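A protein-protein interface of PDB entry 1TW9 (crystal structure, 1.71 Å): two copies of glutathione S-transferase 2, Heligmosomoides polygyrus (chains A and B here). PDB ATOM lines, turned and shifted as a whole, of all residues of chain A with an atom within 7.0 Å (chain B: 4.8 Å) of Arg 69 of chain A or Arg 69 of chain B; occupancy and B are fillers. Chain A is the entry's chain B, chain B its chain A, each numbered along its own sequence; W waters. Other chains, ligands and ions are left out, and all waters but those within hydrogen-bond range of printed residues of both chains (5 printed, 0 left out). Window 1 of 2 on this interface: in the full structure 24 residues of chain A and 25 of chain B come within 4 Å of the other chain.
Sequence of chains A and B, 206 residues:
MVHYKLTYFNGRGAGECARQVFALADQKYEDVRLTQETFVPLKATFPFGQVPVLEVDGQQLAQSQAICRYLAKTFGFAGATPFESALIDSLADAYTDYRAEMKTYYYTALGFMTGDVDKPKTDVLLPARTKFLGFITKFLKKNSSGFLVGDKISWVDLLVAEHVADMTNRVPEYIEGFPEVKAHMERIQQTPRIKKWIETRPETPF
The backbone NH of Ala 66 of chain B lies within hydrogen-bond range of the side-chain carboxylate of Asp 93 of chain A (3.5 Å). The guanidinium group (NH1) of Arg 69 of chain A is in salt-bridge range of the side-chain carboxylate (OD2) of Asp 89 of chain B, at 3.0 Å. OD2 of Asp 89 of chain A is in salt-bridge range of NH1 of Arg 69 of chain B (2.9 Å).
NE of Arg 69 of chain B is in salt-bridge range of OD1 of Asp 89 of chain B (2.8 Å). OD1 of Asp 89 of chain A lies within salt-bridge range of NE of Arg 69 of chain A, at 2.7 Å.
Among the printed residues, pairs that only touch across the chains: Arg 69 of chain A with Arg 69 of chain B, Ala 86 of chain A with Tyr 70 of chain B, Ala 66 of chain A with Asp 89 of chain B, Ser 90 of chain A with Ala 66 of chain B, Asp 89 of chain A with Ala 66 of chain B and Ala 86 of chain A with Ala 66 of chain B.
Of chain B, only Arg 69 (3.5 Å) and Asp 89 (3.0 Å) come within 4 Å of Arg 69 of chain A. Of the printed residues of chain B, Ser 90 of chain A touches Ala 66 (3.8 Å). Of the printed residues of chain B, Asp 93 of chain A touches Ala 66 (3.5 Å). The nearest printed residue of chain B that does not touch Arg 69 of chain A is Lys 73 of chain B (5.7 Å). The nearest printed residue of chain B that does not touch Asp 93 of chain A is Gln 65 of chain B (4.02 Å).
Ala 66 of chain A touches Asp 89 of chain B, and with the chains exchanged Asp 89 of chain A touches Ala 66 of chain B. Arg 69 of chain A touches its own counterpart, Arg 69 of chain B. Arg 69 of chain A touches Asp 89 of chain B, and with the chains exchanged Asp 89 of chain A touches Arg 69 of chain B.
Water W5 lies within hydrogen-bond range of the side-chain carboxylate of Asp 93 of chain A, the guanidinium group of Arg 69 of chain B and the backbone NH of Ala 66 of chain B. Water W1 lies within hydrogen-bond range of OD2 of Asp 89 of chain A (2.7 Å), O of Ala 66 of chain B (2.8 Å) and N of Tyr 70 of chain B (3.4 Å). Water W3 lies within hydrogen-bond range of OD2 of Asp 89 of chain B (2.7 Å), O of Ala 66 of chain A (2.7 Å) and N of Tyr 70 of chain A (3.5 Å). Water W2 bridges N of Gln 65 of chain B and OD2 of Asp 93 of chain A. Water W4 bridges the side-chain amino group (NZ) of Lys 73 of chain A and the side-chain amino group (NZ) of Lys 73 of chain B.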
ATOM      1  N   CYS A  17     -17.367  12.724  33.477  1.00  0.00           N
ATOM      2  CA  CYS A  17     -17.552  12.365  32.091  1.00  0.00           C
ATOM      3  C   CYS A  17     -16.415  12.938  31.235  1.00  0.00           C
ATOM      4  O   CYS A  17     -15.838  12.241  30.389  1.00  0.00           O
ATOM      5  CB  CYS A  17     -18.910  12.834  31.651  1.00  0.00           C
ATOM      6  SG  CYS A  17     -19.333  12.348  29.974  1.00  0.00           S
ATOM      7  N   VAL A  21     -13.800  11.029  28.856  1.00  0.00           N
ATOM      8  CA  VAL A  21     -13.595  11.376  27.456  1.00  0.00           C
ATOM      9  C   VAL A  21     -12.074  11.535  27.203  1.00  0.00           C
ATOM     10  O   VAL A  21     -11.547  10.974  26.238  1.00  0.00           O
ATOM     11  CB  VAL A  21     -14.370  12.640  27.000  1.00  0.00           C
ATOM     12  CG1 VAL A  21     -13.891  13.089  25.574  1.00  0.00           C
ATOM     13  CG2 VAL A  21     -15.858  12.420  27.055  1.00  0.00           C
ATOM     14  N   GLN A  63     -19.397  24.475  32.252  1.00  0.00           N
ATOM     15  CA  GLN A  63     -20.686  23.752  32.218  1.00  0.00           C
ATOM     16  C   GLN A  63     -20.392  22.335  31.745  1.00  0.00           C
ATOM     17  O   GLN A  63     -19.838  22.094  30.645  1.00  0.00           O
ATOM     18  CB  GLN A  63     -21.743  24.424  31.366  1.00  0.00           C
ATOM     19  CG  GLN A  63     -22.173  25.802  31.822  1.00  0.00           C
ATOM     20  CD  GLN A  63     -23.114  25.816  33.036  1.00  0.00           C
ATOM     21  OE1 GLN A  63     -23.224  26.830  33.787  1.00  0.00           O
ATOM     22  NE2 GLN A  63     -23.785  24.718  33.244  1.00  0.00           N
ATOM     23  N   SER A  64     -20.668  21.369  32.632  1.00  0.00           N
ATOM     24  CA  SER A  64     -20.256  19.976  32.366  1.00  0.00           C
ATOM     25  C   SER A  64     -20.625  19.375  31.036  1.00  0.00           C
ATOM     26  O   SER A  64     -19.739  18.782  30.420  1.00  0.00           O
ATOM     27  CB  SER A  64     -20.709  18.999  33.494  1.00  0.00           C
ATOM     28  OG  SER A  64     -22.088  18.992  33.571  1.00  0.00           O
ATOM     29  N   GLN A  65     -21.858  19.527  30.552  1.00  0.00           N
ATOM     30  CA  GLN A  65     -22.222  18.900  29.286  1.00  0.00           C
ATOM     31  C   GLN A  65     -21.601  19.663  28.117  1.00  0.00           C
ATOM     32  O   GLN A  65     -21.218  19.082  27.167  1.00  0.00           O
ATOM     33  CB  GLN A  65     -23.695  18.759  29.051  1.00  0.00           C
ATOM     34  CG  GLN A  65     -24.297  17.602  29.922  1.00  0.00           C
ATOM     35  CD  GLN A  65     -25.649  17.080  29.515  1.00  0.00           C
ATOM     36  OE1 GLN A  65     -26.347  17.544  28.543  1.00  0.00           O
ATOM     37  NE2 GLN A  65     -26.090  16.110  30.304  1.00  0.00           N
ATOM     38  N   ALA A  66     -21.412  20.966  28.279  1.00  0.00           N
ATOM     39  CA  ALA A  66     -20.767  21.755  27.195  1.00  0.00           C
ATOM     40  C   ALA A  66     -19.316  21.287  27.079  1.00  0.00           C
ATOM     41  O   ALA A  66     -18.800  21.145  25.962  1.00  0.00           O
ATOM     42  CB  ALA A  66     -20.861  23.204  27.488  1.00  0.00           C
ATOM     43  N   ILE A  67     -18.659  21.071  28.231  1.00  0.00           N
ATOM     44  CA  ILE A  67     -17.291  20.586  28.233  1.00  0.00           C
ATOM     45  C   ILE A  67     -17.218  19.184  27.616  1.00  0.00           C
ATOM     46  O   ILE A  67     -16.399  18.976  26.749  1.00  0.00           O
ATOM     47  CB  ILE A  67     -16.737  20.558  29.670  1.00  0.00           C
ATOM     48  CG1 ILE A  67     -16.597  21.972  30.223  1.00  0.00           C
ATOM     49  CG2 ILE A  67     -15.405  19.845  29.682  1.00  0.00           C
ATOM     50  CD1 ILE A  67     -16.278  22.067  31.727  1.00  0.00           C
ATOM     51  N   CYS A  68     -18.102  18.256  28.017  1.00  0.00           N
ATOM     52  CA  CYS A  68     -18.071  16.883  27.491  1.00  0.00           C
ATOM     53  C   CYS A  68     -18.284  16.860  26.027  1.00  0.00           C
ATOM     54  O   CYS A  68     -17.617  16.109  25.316  1.00  0.00           O
ATOM     55  CB  CYS A  68     -19.115  15.994  28.133  1.00  0.00           C
ATOM     56  SG  CYS A  68     -18.629  15.735  29.824  1.00  0.00           S
ATOM     57  N   ARG A  69     -19.243  17.636  25.546  1.00  0.00           N
ATOM     58  CA  ARG A  69     -19.562  17.585  24.172  1.00  0.00           C
ATOM     59  C   ARG A  69     -18.410  18.129  23.340  1.00  0.00           C
ATOM     60  O   ARG A  69     -18.134  17.620  22.262  1.00  0.00           O
ATOM     61  CB  ARG A  69     -20.829  18.386  23.881  1.00  0.00           C
ATOM     62  CG  ARG A  69     -21.294  18.400  22.449  1.00  0.00           C
ATOM     63  CD  ARG A  69     -22.523  19.296  22.210  1.00  0.00           C
ATOM     64  NE  ARG A  69     -23.625  18.917  23.081  1.00  0.00           N
ATOM     65  CZ  ARG A  69     -23.965  19.558  24.216  1.00  0.00           C
ATOM     66  NH1 ARG A  69     -23.371  20.681  24.601  1.00  0.00           N
ATOM     67  NH2 ARG A  69     -24.918  19.029  24.972  1.00  0.00           N
ATOM     68  N   TYR A  70     -17.840  19.235  23.815  1.00  0.00           N
ATOM     69  CA  TYR A  70     -16.689  19.887  23.142  1.00  0.00           C
ATOM     70  C   TYR A  70     -15.547  18.879  23.019  1.00  0.00           C
ATOM     71  O   TYR A  70     -14.924  18.717  21.947  1.00  0.00           O
ATOM     72  CB  TYR A  70     -16.211  21.131  23.950  1.00  0.00           C
ATOM     73  CG  TYR A  70     -14.886  21.672  23.450  1.00  0.00           C
ATOM     74  CD1 TYR A  70     -14.787  22.428  22.288  1.00  0.00           C
ATOM     75  CD2 TYR A  70     -13.676  21.371  24.157  1.00  0.00           C
ATOM     76  CE1 TYR A  70     -13.559  22.798  21.809  1.00  0.00           C
ATOM     77  CE2 TYR A  70     -12.440  21.789  23.655  1.00  0.00           C
ATOM     78  CZ  TYR A  70     -12.404  22.493  22.498  1.00  0.00           C
ATOM     79  OH  TYR A  70     -11.217  22.934  21.999  1.00  0.00           O
ATOM     80  N   LEU A  71     -15.234  18.189  24.123  1.00  0.00           N
ATOM     81  CA  LEU A  71     -14.112  17.239  24.094  1.00  0.00           C
ATOM     82  C   LEU A  71     -14.461  16.055  23.220  1.00  0.00           C
ATOM     83  O   LEU A  71     -13.618  15.610  22.458  1.00  0.00           O
ATOM     84  CB  LEU A  71     -13.794  16.793  25.489  1.00  0.00           C
ATOM     85  CG  LEU A  71     -13.243  17.870  26.426  1.00  0.00           C
ATOM     86  CD1 LEU A  71     -13.148  17.324  27.845  1.00  0.00           C
ATOM     87  CD2 LEU A  71     -11.912  18.343  25.887  1.00  0.00           C
ATOM     88  N   ALA A  72     -15.711  15.563  23.294  1.00  0.00           N
ATOM     89  CA  ALA A  72     -16.129  14.457  22.461  1.00  0.00           C
ATOM     90  C   ALA A  72     -16.053  14.774  20.992  1.00  0.00           C
ATOM     91  O   ALA A  72     -15.603  13.932  20.167  1.00  0.00           O
ATOM     92  CB  ALA A  72     -17.515  14.018  22.830  1.00  0.00           C
ATOM     93  N   LYS A  73     -16.470  15.959  20.609  1.00  0.00           N
ATOM     94  CA  LYS A  73     -16.402  16.306  19.198  1.00  0.00           C
ATOM     95  C   LYS A  73     -14.949  16.416  18.769  1.00  0.00           C
ATOM     96  O   LYS A  73     -14.561  16.037  17.684  1.00  0.00           O
ATOM     97  CB  LYS A  73     -17.149  17.565  18.920  1.00  0.00           C
ATOM     98  CG  LYS A  73     -18.641  17.388  18.884  1.00  0.00           C
ATOM     99  CD  LYS A  73     -19.343  18.759  18.879  1.00  0.00           C
ATOM    100  CE  LYS A  73     -20.834  18.591  18.778  1.00  0.00           C
ATOM    101  NZ  LYS A  73     -21.173  18.042  17.466  1.00  0.00           N
ATOM    102  N   THR A  74     -14.126  16.955  19.637  1.00  0.00           N
ATOM    103  CA  THR A  74     -12.663  17.101  19.339  1.00  0.00           C
ATOM    104  C   THR A  74     -12.020  15.745  19.068  1.00  0.00           C
ATOM    105  O   THR A  74     -11.194  15.583  18.159  1.00  0.00           O
ATOM    106  CB  THR A  74     -11.977  17.716  20.515  1.00  0.00           C
ATOM    107  OG1 THR A  74     -12.425  19.087  20.738  1.00  0.00           O
ATOM    108  CG2 THR A  74     -10.492  17.832  20.274  1.00  0.00           C
ATOM    109  N   PHE A  75     -12.397  14.746  19.859  1.00  0.00           N
ATOM    110  CA  PHE A  75     -11.760  13.416  19.816  1.00  0.00           C
ATOM    111  C   PHE A  75     -12.510  12.289  19.111  1.00  0.00           C
ATOM    112  O   PHE A  75     -11.966  11.200  18.976  1.00  0.00           O
ATOM    113  CB  PHE A  75     -11.370  13.018  21.206  1.00  0.00           C
ATOM    114  CG  PHE A  75     -10.416  13.966  21.828  1.00  0.00           C
ATOM    115  CD1 PHE A  75     -10.730  14.652  22.987  1.00  0.00           C
ATOM    116  CD2 PHE A  75      -9.182  14.158  21.259  1.00  0.00           C
ATOM    117  CE1 PHE A  75      -9.793  15.577  23.552  1.00  0.00           C
ATOM    118  CE2 PHE A  75      -8.255  15.072  21.835  1.00  0.00           C
ATOM    119  CZ  PHE A  75      -8.592  15.776  22.957  1.00  0.00           C
ATOM    120  N   PHE A  77     -15.968  11.312  19.591  1.00  0.00           N
ATOM    121  CA  PHE A  77     -16.917  10.476  20.419  1.00  0.00           C
ATOM    122  C   PHE A  77     -18.277  11.147  20.542  1.00  0.00           C
ATOM    123  O   PHE A  77     -18.960  11.063  21.593  1.00  0.00           O
ATOM    124  CB  PHE A  77     -16.334  10.152  21.786  1.00  0.00           C
ATOM    125  CG  PHE A  77     -15.023   9.462  21.700  1.00  0.00           C
ATOM    126  CD1 PHE A  77     -13.858  10.057  22.153  1.00  0.00           C
ATOM    127  CD2 PHE A  77     -14.942   8.228  21.084  1.00  0.00           C
ATOM    128  CE1 PHE A  77     -12.619   9.363  22.019  1.00  0.00           C
ATOM    129  CE2 PHE A  77     -13.729   7.550  20.947  1.00  0.00           C
ATOM    130  CZ  PHE A  77     -12.565   8.167  21.379  1.00  0.00           C
ATOM    131  N   ALA A  78     -18.634  11.892  19.500  1.00  0.00           N
ATOM    132  CA  ALA A  78     -19.929  12.589  19.519  1.00  0.00           C
ATOM    133  C   ALA A  78     -20.710  12.253  18.291  1.00  0.00           C
ATOM    134  O   ALA A  78     -21.406  13.120  17.716  1.00  0.00           O
ATOM    135  CB  ALA A  78     -19.751  14.054  19.638  1.00  0.00           C
ATOM    136  N   SER A  85     -25.130  13.225  16.486  1.00  0.00           N
ATOM    137  CA  SER A  85     -24.692  14.110  17.568  1.00  0.00           C
ATOM    138  C   SER A  85     -25.908  14.652  18.350  1.00  0.00           C
ATOM    139  O   SER A  85     -25.907  14.735  19.615  1.00  0.00           O
ATOM    140  CB  SER A  85     -23.831  15.249  17.031  1.00  0.00           C
ATOM    141  OG  SER A  85     -23.179  15.865  18.125  1.00  0.00           O
ATOM    142  N   ALA A  86     -26.944  14.992  17.622  1.00  0.00           N
ATOM    143  CA  ALA A  86     -28.144  15.546  18.245  1.00  0.00           C
ATOM    144  C   ALA A  86     -28.852  14.480  19.073  1.00  0.00           C
ATOM    145  O   ALA A  86     -29.336  14.754  20.144  1.00  0.00           O
ATOM    146  CB  ALA A  86     -29.054  16.118  17.218  1.00  0.00           C
ATOM    147  N   ILE A  88     -27.473  11.919  20.576  1.00  0.00           N
ATOM    148  CA  ILE A  88     -26.608  11.782  21.758  1.00  0.00           C
ATOM    149  C   ILE A  88     -26.909  12.925  22.751  1.00  0.00           C
ATOM    150  O   ILE A  88     -27.144  12.685  23.939  1.00  0.00           O
ATOM    151  CB  ILE A  88     -25.145  11.823  21.308  1.00  0.00           C
ATOM    152  CG1 ILE A  88     -24.800  10.461  20.559  1.00  0.00           C
ATOM    153  CG2 ILE A  88     -24.222  12.136  22.447  1.00  0.00           C
ATOM    154  CD1 ILE A  88     -23.609  10.536  19.720  1.00  0.00           C
ATOM    155  N   ASP A  89     -27.000  14.131  22.250  1.00  0.00           N
ATOM    156  CA  ASP A  89     -27.376  15.291  23.073  1.00  0.00           C
ATOM    157  C   ASP A  89     -28.763  15.096  23.723  1.00  0.00           C
ATOM    158  O   ASP A  89     -28.968  15.418  24.877  1.00  0.00           O
ATOM    159  CB  ASP A  89     -27.499  16.536  22.230  1.00  0.00           C
ATOM    160  CG  ASP A  89     -26.194  17.100  21.759  1.00  0.00           C
ATOM    161  OD1 ASP A  89     -25.124  16.768  22.343  1.00  0.00           O
ATOM    162  OD2 ASP A  89     -26.189  18.033  20.886  1.00  0.00           O
ATOM    163  N   SER A  90     -29.709  14.591  22.970  1.00  0.00           N
ATOM    164  CA  SER A  90     -31.064  14.380  23.531  1.00  0.00           C
ATOM    165  C   SER A  90     -31.073  13.381  24.685  1.00  0.00           C
ATOM    166  O   SER A  90     -31.824  13.585  25.621  1.00  0.00           O
ATOM    167  CB  SER A  90     -32.049  13.955  22.459  1.00  0.00           C
ATOM    168  OG  SER A  90     -31.916  12.602  22.027  1.00  0.00           O
ATOM    169  N   ALA A  92     -28.497  12.750  26.537  1.00  0.00           N
ATOM    170  CA  ALA A  92     -27.800  13.409  27.640  1.00  0.00           C
ATOM    171  C   ALA A  92     -28.689  14.435  28.379  1.00  0.00           C
ATOM    172  O   ALA A  92     -28.584  14.590  29.569  1.00  0.00           O
ATOM    173  CB  ALA A  92     -26.502  14.046  27.214  1.00  0.00           C
ATOM    174  N   ASP A  93     -29.588  15.083  27.662  1.00  0.00           N
ATOM    175  CA  ASP A  93     -30.579  15.993  28.224  1.00  0.00           C
ATOM    176  C   ASP A  93     -31.608  15.205  29.052  1.00  0.00           C
ATOM    177  O   ASP A  93     -32.019  15.617  30.132  1.00  0.00           O
ATOM    178  CB  ASP A  93     -31.273  16.709  27.072  1.00  0.00           C
ATOM    179  CG  ASP A  93     -30.581  18.008  26.636  1.00  0.00           C
ATOM    180  OD1 ASP A  93     -29.721  18.513  27.413  1.00  0.00           O
ATOM    181  OD2 ASP A  93     -30.853  18.602  25.525  1.00  0.00           O
ATOM    182  N   TRP A 155     -19.855  10.015  24.133  1.00  0.00           N
ATOM    183  CA  TRP A 155     -19.834  10.568  25.462  1.00  0.00           C
ATOM    184  C   TRP A 155     -21.091  10.277  26.296  1.00  0.00           C
ATOM    185  O   TRP A 155     -20.995  10.146  27.531  1.00  0.00           O
ATOM    186  CB  TRP A 155     -19.500  12.012  25.461  1.00  0.00           C
ATOM    187  CG  TRP A 155     -20.522  12.947  24.840  1.00  0.00           C
ATOM    188  CD1 TRP A 155     -20.657  13.265  23.510  1.00  0.00           C
ATOM    189  CD2 TRP A 155     -21.496  13.743  25.543  1.00  0.00           C
ATOM    190  NE1 TRP A 155     -21.681  14.174  23.350  1.00  0.00           N
ATOM    191  CE2 TRP A 155     -22.207  14.498  24.571  1.00  0.00           C
ATOM    192  CE3 TRP A 155     -21.856  13.893  26.893  1.00  0.00           C
ATOM    193  CZ2 TRP A 155     -23.219  15.403  24.921  1.00  0.00           C
ATOM    194  CZ3 TRP A 155     -22.864  14.773  27.212  1.00  0.00           C
ATOM    195  CH2 TRP A 155     -23.492  15.543  26.253  1.00  0.00           C
ATOM    196  N   GLN B  65     -33.115  21.861  23.881  1.00  0.00           N
ATOM    197  CA  GLN B  65     -31.813  22.387  23.516  1.00  0.00           C
ATOM    198  C   GLN B  65     -31.139  21.488  22.465  1.00  0.00           C
ATOM    199  O   GLN B  65     -30.394  21.986  21.642  1.00  0.00           O
ATOM    200  CB  GLN B  65     -30.885  22.535  24.704  1.00  0.00           C
ATOM    201  CG  GLN B  65     -31.250  23.777  25.498  1.00  0.00           C
ATOM    202  CD  GLN B  65     -30.253  24.345  26.462  1.00  0.00           C
ATOM    203  OE1 GLN B  65     -29.102  23.856  26.669  1.00  0.00           O
ATOM    204  NE2 GLN B  65     -30.752  25.375  27.193  1.00  0.00           N
ATOM    205  N   ALA B  66     -31.406  20.184  22.468  1.00  0.00           N
ATOM    206  CA  ALA B  66     -30.806  19.283  21.440  1.00  0.00           C
ATOM    207  C   ALA B  66     -31.318  19.644  20.022  1.00  0.00           C
ATOM    208  O   ALA B  66     -30.588  19.646  19.073  1.00  0.00           O
ATOM    209  CB  ALA B  66     -31.097  17.888  21.748  1.00  0.00           C
ATOM    210  N   ILE B  67     -32.594  19.916  19.992  1.00  0.00           N
ATOM    211  CA  ILE B  67     -33.297  20.378  18.817  1.00  0.00           C
ATOM    212  C   ILE B  67     -32.714  21.712  18.304  1.00  0.00           C
ATOM    213  O   ILE B  67     -32.364  21.844  17.121  1.00  0.00           O
ATOM    214  CB  ILE B  67     -34.794  20.460  19.095  1.00  0.00           C
ATOM    215  CG1 ILE B  67     -35.419  19.059  19.266  1.00  0.00           C
ATOM    216  CG2 ILE B  67     -35.448  21.199  17.970  1.00  0.00           C
ATOM    217  CD1 ILE B  67     -36.829  19.168  19.759  1.00  0.00           C
ATOM    218  N   CYS B  68     -32.602  22.695  19.184  1.00  0.00           N
ATOM    219  CA  CYS B  68     -32.135  24.047  18.806  1.00  0.00           C
ATOM    220  C   CYS B  68     -30.708  23.955  18.299  1.00  0.00           C
ATOM    221  O   CYS B  68     -30.399  24.530  17.311  1.00  0.00           O
ATOM    222  CB  CYS B  68     -32.172  24.965  20.017  1.00  0.00           C
ATOM    223  SG  CYS B  68     -33.871  25.378  20.321  1.00  0.00           S
ATOM    224  N   ARG B  69     -29.839  23.238  19.021  1.00  0.00           N
ATOM    225  CA  ARG B  69     -28.418  23.133  18.625  1.00  0.00           C
ATOM    226  C   ARG B  69     -28.313  22.439  17.293  1.00  0.00           C
ATOM    227  O   ARG B  69     -27.616  22.894  16.420  1.00  0.00           O
ATOM    228  CB  ARG B  69     -27.643  22.416  19.662  1.00  0.00           C
ATOM    229  CG  ARG B  69     -26.179  22.277  19.395  1.00  0.00           C
ATOM    230  CD  ARG B  69     -25.384  21.468  20.394  1.00  0.00           C
ATOM    231  NE  ARG B  69     -25.594  21.907  21.748  1.00  0.00           N
ATOM    232  CZ  ARG B  69     -26.485  21.427  22.607  1.00  0.00           C
ATOM    233  NH1 ARG B  69     -27.201  20.321  22.354  1.00  0.00           N
ATOM    234  NH2 ARG B  69     -26.577  22.011  23.802  1.00  0.00           N
ATOM    235  N   TYR B  70     -29.078  21.391  17.098  1.00  0.00           N
ATOM    236  CA  TYR B  70     -29.104  20.693  15.815  1.00  0.00           C
ATOM    237  C   TYR B  70     -29.492  21.618  14.631  1.00  0.00           C
ATOM    238  O   TYR B  70     -28.814  21.682  13.619  1.00  0.00           O
ATOM    239  CB  TYR B  70     -30.048  19.488  15.888  1.00  0.00           C
ATOM    240  CG  TYR B  70     -30.322  18.869  14.527  1.00  0.00           C
ATOM    241  CD1 TYR B  70     -29.367  18.019  13.936  1.00  0.00           C
ATOM    242  CD2 TYR B  70     -31.475  19.118  13.809  1.00  0.00           C
ATOM    243  CE1 TYR B  70     -29.521  17.544  12.727  1.00  0.00           C
ATOM    244  CE2 TYR B  70     -31.617  18.598  12.620  1.00  0.00           C
ATOM    245  CZ  TYR B  70     -30.701  17.763  12.090  1.00  0.00           C
ATOM    246  OH  TYR B  70     -30.962  17.297  10.788  1.00  0.00           O
ATOM    247  N   LEU B  71     -30.635  22.287  14.782  1.00  0.00           N
ATOM    248  CA  LEU B  71     -31.129  23.238  13.800  1.00  0.00           C
ATOM    249  C   LEU B  71     -30.151  24.334  13.606  1.00  0.00           C
ATOM    250  O   LEU B  71     -29.820  24.692  12.490  1.00  0.00           O
ATOM    251  CB  LEU B  71     -32.462  23.773  14.240  1.00  0.00           C
ATOM    252  CG  LEU B  71     -33.599  22.796  14.180  1.00  0.00           C
ATOM    253  CD1 LEU B  71     -34.860  23.430  14.774  1.00  0.00           C
ATOM    254  CD2 LEU B  71     -33.821  22.154  12.770  1.00  0.00           C
ATOM    255  N   ALA B  72     -29.581  24.831  14.702  1.00  0.00           N
ATOM    256  CA  ALA B  72     -28.586  25.930  14.603  1.00  0.00           C
ATOM    257  C   ALA B  72     -27.300  25.570  13.863  1.00  0.00           C
ATOM    258  O   ALA B  72     -26.858  26.287  13.026  1.00  0.00           O
ATOM    259  CB  ALA B  72     -28.265  26.487  15.955  1.00  0.00           C
ATOM    260  N   LYS B  73     -26.834  24.345  14.030  1.00  0.00           N
ATOM    261  CA  LYS B  73     -25.681  23.860  13.306  1.00  0.00           C
ATOM    262  C   LYS B  73     -26.041  23.646  11.823  1.00  0.00           C
ATOM    263  O   LYS B  73     -25.187  23.849  10.941  1.00  0.00           O
ATOM    264  CB  LYS B  73     -25.164  22.619  13.940  1.00  0.00           C
ATOM    265  CG  LYS B  73     -24.465  22.916  15.242  1.00  0.00           C
ATOM    266  CD  LYS B  73     -23.971  21.644  16.028  1.00  0.00           C
ATOM    267  CE  LYS B  73     -23.024  21.914  17.218  1.00  0.00           C
ATOM    268  NZ  LYS B  73     -21.629  22.382  16.806  1.00  0.00           N
ATOM    269  N   ASP B  89     -23.061  26.802  23.871  1.00  0.00           N
ATOM    270  CA  ASP B  89     -23.612  25.727  24.710  1.00  0.00           C
ATOM    271  C   ASP B  89     -23.530  26.100  26.173  1.00  0.00           C
ATOM    272  O   ASP B  89     -24.482  25.885  26.926  1.00  0.00           O
ATOM    273  CB  ASP B  89     -22.884  24.418  24.540  1.00  0.00           C
ATOM    274  CG  ASP B  89     -23.089  23.776  23.231  1.00  0.00           C
ATOM    275  OD1 ASP B  89     -24.057  24.139  22.499  1.00  0.00           O
ATOM    276  OD2 ASP B  89     -22.370  22.835  22.823  1.00  0.00           O
ATOM    277  N   TRP B 155     -28.013  30.670  18.259  1.00  0.00           N
ATOM    278  CA  TRP B 155     -29.312  30.231  18.902  1.00  0.00           C
ATOM    279  C   TRP B 155     -29.390  30.649  20.362  1.00  0.00           C
ATOM    280  O   TRP B 155     -30.526  30.897  20.878  1.00  0.00           O
ATOM    281  CB  TRP B 155     -29.503  28.738  18.771  1.00  0.00           C
ATOM    282  CG  TRP B 155     -28.483  27.867  19.429  1.00  0.00           C
ATOM    283  CD1 TRP B 155     -27.241  27.493  18.947  1.00  0.00           C
ATOM    284  CD2 TRP B 155     -28.678  27.114  20.636  1.00  0.00           C
ATOM    285  NE1 TRP B 155     -26.653  26.583  19.815  1.00  0.00           N
ATOM    286  CE2 TRP B 155     -27.494  26.377  20.880  1.00  0.00           C
ATOM    287  CE3 TRP B 155     -29.677  27.094  21.601  1.00  0.00           C
ATOM    288  CZ2 TRP B 155     -27.325  25.566  22.009  1.00  0.00           C
ATOM    289  CZ3 TRP B 155     -29.507  26.261  22.696  1.00  0.00           C
ATOM    290  CH2 TRP B 155     -28.358  25.514  22.884  1.00  0.00           C
HETATM  291  O   HOH W   1     -27.954  18.807  19.049  1.00  0.00           O
HETATM  292  O   HOH W   2     -33.051  20.419  26.291  1.00  0.00           O
HETATM  293  O   HOH W   3     -19.978  22.000  23.649  1.00  0.00           O
HETATM  294  O   HOH W   4     -20.540  20.053  15.555  1.00  0.00           O
HETATM  295  O   HOH W   5     -28.755  19.198  24.520  1.00  0.00           O
